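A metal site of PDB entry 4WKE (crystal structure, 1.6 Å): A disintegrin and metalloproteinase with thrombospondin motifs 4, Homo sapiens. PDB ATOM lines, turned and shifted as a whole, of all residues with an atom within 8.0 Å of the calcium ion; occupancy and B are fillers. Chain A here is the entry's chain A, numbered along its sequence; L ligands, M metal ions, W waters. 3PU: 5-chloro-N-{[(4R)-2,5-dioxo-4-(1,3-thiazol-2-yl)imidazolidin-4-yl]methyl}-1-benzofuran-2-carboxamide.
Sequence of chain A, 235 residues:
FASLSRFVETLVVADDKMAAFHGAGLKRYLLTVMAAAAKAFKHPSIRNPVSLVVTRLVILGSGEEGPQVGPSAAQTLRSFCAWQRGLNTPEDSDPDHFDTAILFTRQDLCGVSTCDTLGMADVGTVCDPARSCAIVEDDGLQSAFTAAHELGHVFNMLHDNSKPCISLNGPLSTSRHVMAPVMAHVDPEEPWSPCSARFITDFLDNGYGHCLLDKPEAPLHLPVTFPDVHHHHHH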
ATOM      1  N   PRO A  71     -16.835 -18.534  -0.249  1.00  0.00           N
ATOM      2  CA  PRO A  71     -15.746 -19.511  -0.199  1.00  0.00           C
ATOM      3  C   PRO A  71     -15.071 -19.598   1.170  1.00  0.00           C
ATOM      4  O   PRO A  71     -14.738 -20.691   1.608  1.00  0.00           O
ATOM      5  CB  PRO A  71     -14.750 -19.011  -1.253  1.00  0.00           C
ATOM      6  CG  PRO A  71     -15.531 -18.130  -2.162  1.00  0.00           C
ATOM      7  CD  PRO A  71     -16.660 -17.571  -1.359  1.00  0.00           C
ATOM      8  N   ALA A  73     -14.588 -20.313   4.665  1.00  0.00           N
ATOM      9  CA  ALA A  73     -15.293 -21.016   5.731  1.00  0.00           C
ATOM     10  C   ALA A  73     -15.376 -20.148   6.990  1.00  0.00           C
ATOM     11  O   ALA A  73     -16.447 -20.044   7.607  1.00  0.00           O
ATOM     12  CB  ALA A  73     -14.619 -22.338   6.044  1.00  0.00           C
ATOM     13  N   ARG A 106     -24.461 -25.614  -0.190  1.00  0.00           N
ATOM     14  CA  ARG A 106     -23.776 -26.255  -1.315  1.00  0.00           C
ATOM     15  C   ARG A 106     -22.518 -25.485  -1.706  1.00  0.00           C
ATOM     16  O   ARG A 106     -21.768 -25.931  -2.581  1.00  0.00           O
ATOM     17  CB  ARG A 106     -24.696 -26.377  -2.531  1.00  0.00           C
ATOM     18  CG  ARG A 106     -26.002 -27.119  -2.310  1.00  0.00           C
ATOM     19  CD  ARG A 106     -25.813 -28.620  -2.215  1.00  0.00           C
ATOM     20  NE  ARG A 106     -25.538 -29.231  -3.519  1.00  0.00           N
ATOM     21  CZ  ARG A 106     -25.427 -30.535  -3.734  1.00  0.00           C
ATOM     22  NH1 ARG A 106     -25.165 -30.987  -4.959  1.00  0.00           N
ATOM     23  NH2 ARG A 106     -25.578 -31.399  -2.732  1.00  0.00           N
ATOM     24  N   GLN A 107     -22.287 -24.324  -1.092  1.00  0.00           N
ATOM     25  CA  GLN A 107     -21.052 -23.567  -1.334  1.00  0.00           C
ATOM     26  C   GLN A 107     -19.836 -24.430  -1.023  1.00  0.00           C
ATOM     27  O   GLN A 107     -19.802 -25.130  -0.012  1.00  0.00           O
ATOM     28  CB  GLN A 107     -21.026 -22.297  -0.468  1.00  0.00           C
ATOM     29  CG  GLN A 107     -19.726 -21.500  -0.514  1.00  0.00           C
ATOM     30  CD  GLN A 107     -19.487 -20.830  -1.851  1.00  0.00           C
ATOM     31  OE1 GLN A 107     -20.334 -20.082  -2.333  1.00  0.00           O
ATOM     32  NE2 GLN A 107     -18.338 -21.097  -2.461  1.00  0.00           N
ATOM     33  N   ASP A 108     -18.843 -24.392  -1.911  1.00  0.00           N
ATOM     34  CA  ASP A 108     -17.565 -25.050  -1.655  1.00  0.00           C
ATOM     35  C   ASP A 108     -16.790 -24.196  -0.662  1.00  0.00           C
ATOM     36  O   ASP A 108     -16.220 -23.170  -1.020  1.00  0.00           O
ATOM     37  CB  ASP A 108     -16.780 -25.244  -2.970  1.00  0.00           C
ATOM     38  CG  ASP A 108     -15.471 -25.992  -2.766  1.00  0.00           C
ATOM     39  OD1 ASP A 108     -15.131 -26.369  -1.631  1.00  0.00           O
ATOM     40  OD2 ASP A 108     -14.750 -26.200  -3.782  1.00  0.00           O
ATOM     41  N   LEU A 109     -16.768 -24.630   0.597  1.00  0.00           N
ATOM     42  CA  LEU A 109     -16.100 -23.878   1.665  1.00  0.00           C
ATOM     43  C   LEU A 109     -14.611 -24.105   1.601  1.00  0.00           C
ATOM     44  O   LEU A 109     -14.166 -25.203   1.276  1.00  0.00           O
ATOM     45  CB  LEU A 109     -16.618 -24.347   3.032  1.00  0.00           C
ATOM     46  CG  LEU A 109     -18.116 -24.158   3.268  1.00  0.00           C
ATOM     47  CD1 LEU A 109     -18.491 -24.815   4.579  1.00  0.00           C
ATOM     48  CD2 LEU A 109     -18.509 -22.686   3.254  1.00  0.00           C
ATOM     49  N   CYS A 110     -13.852 -23.059   1.901  1.00  0.00           N
ATOM     50  CA  CYS A 110     -12.395 -23.121   1.822  1.00  0.00           C
ATOM     51  C   CYS A 110     -11.684 -22.597   3.066  1.00  0.00           C
ATOM     52  O   CYS A 110     -12.244 -21.818   3.850  1.00  0.00           O
ATOM     53  CB  CYS A 110     -11.899 -22.343   0.593  1.00  0.00           C
ATOM     54  SG  CYS A 110     -12.775 -22.707  -0.948  1.00  0.00           S
ATOM     55  N   GLY A 111     -10.459 -23.072   3.242  1.00  0.00           N
ATOM     56  CA  GLY A 111      -9.506 -22.523   4.200  1.00  0.00           C
ATOM     57  C   GLY A 111      -8.609 -21.521   3.503  1.00  0.00           C
ATOM     58  O   GLY A 111      -8.932 -21.001   2.441  1.00  0.00           O
ATOM     59  N   THR A 114      -6.372 -24.199   0.658  1.00  0.00           N
ATOM     60  CA  THR A 114      -7.128 -25.217  -0.056  1.00  0.00           C
ATOM     61  C   THR A 114      -8.630 -25.074   0.219  1.00  0.00           C
ATOM     62  O   THR A 114      -9.030 -24.410   1.176  1.00  0.00           O
ATOM     63  CB  THR A 114      -6.691 -26.646   0.342  1.00  0.00           C
ATOM     64  OG1 THR A 114      -7.029 -26.908   1.706  1.00  0.00           O
ATOM     65  CG2 THR A 114      -5.198 -26.835   0.141  1.00  0.00           C
ATOM     66  N   CYS A 115      -9.418 -25.705  -0.636  1.00  0.00           N
ATOM     67  CA  CYS A 115     -10.869 -25.805  -0.452  1.00  0.00           C
ATOM     68  C   CYS A 115     -11.297 -27.207  -0.036  1.00  0.00           C
ATOM     69  O   CYS A 115     -12.454 -27.580  -0.190  1.00  0.00           O
ATOM     70  CB  CYS A 115     -11.598 -25.396  -1.730  1.00  0.00           C
ATOM     71  SG  CYS A 115     -11.387 -23.642  -2.111  1.00  0.00           S
ATOM     72  N   ASP A 116     -10.367 -27.973   0.508  1.00  0.00           N
ATOM     73  CA  ASP A 116     -10.639 -29.340   0.962  1.00  0.00           C
ATOM     74  C   ASP A 116     -11.598 -29.382   2.152  1.00  0.00           C
ATOM     75  O   ASP A 116     -12.281 -30.393   2.349  1.00  0.00           O
ATOM     76  CB  ASP A 116      -9.336 -30.031   1.364  1.00  0.00           C
ATOM     77  CG  ASP A 116      -8.424 -30.304   0.179  1.00  0.00           C
ATOM     78  OD1 ASP A 116      -8.822 -30.031  -0.978  1.00  0.00           O
ATOM     79  OD2 ASP A 116      -7.303 -30.776   0.419  1.00  0.00           O
ATOM     80  N   THR A 117     -11.653 -28.315   2.933  1.00  0.00           N
ATOM     81  CA  THR A 117     -12.519 -28.292   4.122  1.00  0.00           C
ATOM     82  C   THR A 117     -13.989 -28.527   3.748  1.00  0.00           C
ATOM     83  O   THR A 117     -14.456 -28.089   2.691  1.00  0.00           O
ATOM     84  CB  THR A 117     -12.418 -26.994   4.948  1.00  0.00           C
ATOM     85  OG1 THR A 117     -13.264 -27.089   6.108  1.00  0.00           O
ATOM     86  CG2 THR A 117     -12.792 -25.769   4.138  1.00  0.00           C
ATOM     87  N   LEU A 118     -14.724 -29.190   4.645  1.00  0.00           N
ATOM     88  CA  LEU A 118     -16.145 -29.463   4.454  1.00  0.00           C
ATOM     89  C   LEU A 118     -17.014 -28.771   5.503  1.00  0.00           C
ATOM     90  O   LEU A 118     -18.221 -28.921   5.468  1.00  0.00           O
ATOM     91  CB  LEU A 118     -16.393 -30.975   4.506  1.00  0.00           C
ATOM     92  CG  LEU A 118     -15.808 -31.802   3.344  1.00  0.00           C
ATOM     93  CD1 LEU A 118     -15.955 -33.281   3.670  1.00  0.00           C
ATOM     94  CD2 LEU A 118     -16.519 -31.452   2.065  1.00  0.00           C
ATOM     95  N   GLY A 119     -16.418 -28.003   6.416  1.00  0.00           N
ATOM     96  CA  GLY A 119     -17.200 -27.398   7.491  1.00  0.00           C
ATOM     97  C   GLY A 119     -16.325 -26.650   8.476  1.00  0.00           C
ATOM     98  O   GLY A 119     -15.088 -26.732   8.413  1.00  0.00           O
ATOM     99  N   GLU A 137     -20.603 -27.979   4.496  1.00  0.00           N
ATOM    100  CA  GLU A 137     -20.705 -28.102   3.048  1.00  0.00           C
ATOM    101  C   GLU A 137     -21.365 -29.438   2.741  1.00  0.00           C
ATOM    102  O   GLU A 137     -20.827 -30.502   3.076  1.00  0.00           O
ATOM    103  CB  GLU A 137     -19.319 -28.027   2.416  1.00  0.00           C
ATOM    104  CG  GLU A 137     -19.309 -28.275   0.916  1.00  0.00           C
ATOM    105  CD  GLU A 137     -17.922 -28.265   0.337  1.00  0.00           C
ATOM    106  OE1 GLU A 137     -17.040 -27.558   0.872  1.00  0.00           O
ATOM    107  OE2 GLU A 137     -17.695 -28.985  -0.666  1.00  0.00           O
HETATM  108  C7  3PU L   1     -11.338 -29.397   7.879  1.00  0.00           C
HETATM  109  C6  3PU L   1     -14.869 -32.944   7.975  1.00  0.00           C
HETATM  110  C1  3PU L   1     -13.721 -36.322  10.012  1.00  0.00           C
HETATM  111  C5  3PU L   1     -15.563 -35.346   8.776  1.00  0.00           C
HETATM  112  C4  3PU L   1     -10.439 -24.665   8.375  1.00  0.00           C
HETATM  113  C3  3PU L   1      -9.461 -25.525   7.940  1.00  0.00           C
HETATM  114  C2  3PU L   1     -12.916 -35.227   9.863  1.00  0.00           C
HETATM  115  C8  3PU L   1     -14.996 -36.386   9.495  1.00  0.00           C
HETATM  116  C9  3PU L   1     -13.493 -34.215   9.145  1.00  0.00           C
HETATM  117  C10 3PU L   1     -14.760 -34.219   8.606  1.00  0.00           C
HETATM  118  C11 3PU L   1     -13.677 -32.269   8.180  1.00  0.00           C
HETATM  119  C12 3PU L   1     -10.898 -27.032   8.643  1.00  0.00           C
HETATM  120  C13 3PU L   1     -10.872 -28.894  10.207  1.00  0.00           C
HETATM  121  C14 3PU L   1     -13.084 -28.707  10.633  1.00  0.00           C
HETATM  122  C15 3PU L   1     -13.202 -30.977   7.790  1.00  0.00           C
HETATM  123  C16 3PU L   1     -11.505 -28.347   8.959  1.00  0.00           C
HETATM  124  N17 3PU L   1      -9.721 -26.863   8.088  1.00  0.00           N
HETATM  125  N18 3PU L   1     -11.882 -29.138  11.097  1.00  0.00           N
HETATM  126  N19 3PU L   1     -12.879 -28.211   9.386  1.00  0.00           N
HETATM  127  N20 3PU L   1     -11.952 -30.654   8.259  1.00  0.00           N
HETATM  128  O21 3PU L   1      -9.680 -29.077  10.373  1.00  0.00           O
HETATM  129  O22 3PU L   1     -14.141 -28.780  11.244  1.00  0.00           O
HETATM  130  O23 3PU L   1     -13.878 -30.215   7.110  1.00  0.00           O
HETATM  131  O24 3PU L   1     -12.835 -33.061   8.902  1.00  0.00           O
HETATM  132  S25 3PU L   1     -11.749 -25.584   9.024  1.00  0.00           S
HETATM  133 CL2  3PU L   1     -15.802 -37.884   9.826  1.00  0.00          CL
HETATM  134 CA    CA M   1     -14.696 -27.374   0.400  1.00  0.00          CA
HETATM  135  O   HOH W   1     -14.824 -29.493  -0.544  1.00  0.00           O
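The calcium ion is bound by the side-chain carboxylate (OD1) of Asp 108 (2.3 Å), water W1 (2.3 Å), the backbone carbonyl oxygen (O) of Cys 115 (2.3 Å), the side-chain carboxylate (OE1) of Glu 137 (2.4 Å), the backbone carbonyl oxygen (O) of Leu 109 (2.4 Å) and the backbone carbonyl oxygen (O) of Thr 117 (2.4 Å).
The side-chain hydroxyl (OG1) of Thr 117 is in hydrogen-bond range of an oxygen (O23) of the ligand, at 3.3 Å. The backbone NH of Leu 118 sits at hydrogen-bond distance from an oxygen (O23) of the ligand (2.8 Å). The backbone NH (N) of Gly 119 is in hydrogen-bond range of an oxygen (O23) of the ligand, at 3.4 Å. The backbone carbonyl oxygen (O) of Gly 119 is in hydrogen-bond range of a nitrogen (N19) of the ligand (2.8 Å).
Of the 15 residues printed, 5 come within 4 Å of the calcium ion. The nearest printed residue that does not touch the calcium ion is Asp 116 (4.1 Å).
SG of Cys 110 forms a disulfide with SG of Cys 115, at 2.0 Å. The backbone NH (N) of Glu 137 lies within hydrogen-bond range of the backbone carbonyl oxygen (O) of Leu 118 (2.7 Å). O of Gly 119 lies within hydrogen-bond range of OG1 of Thr 117 (3.0 Å).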
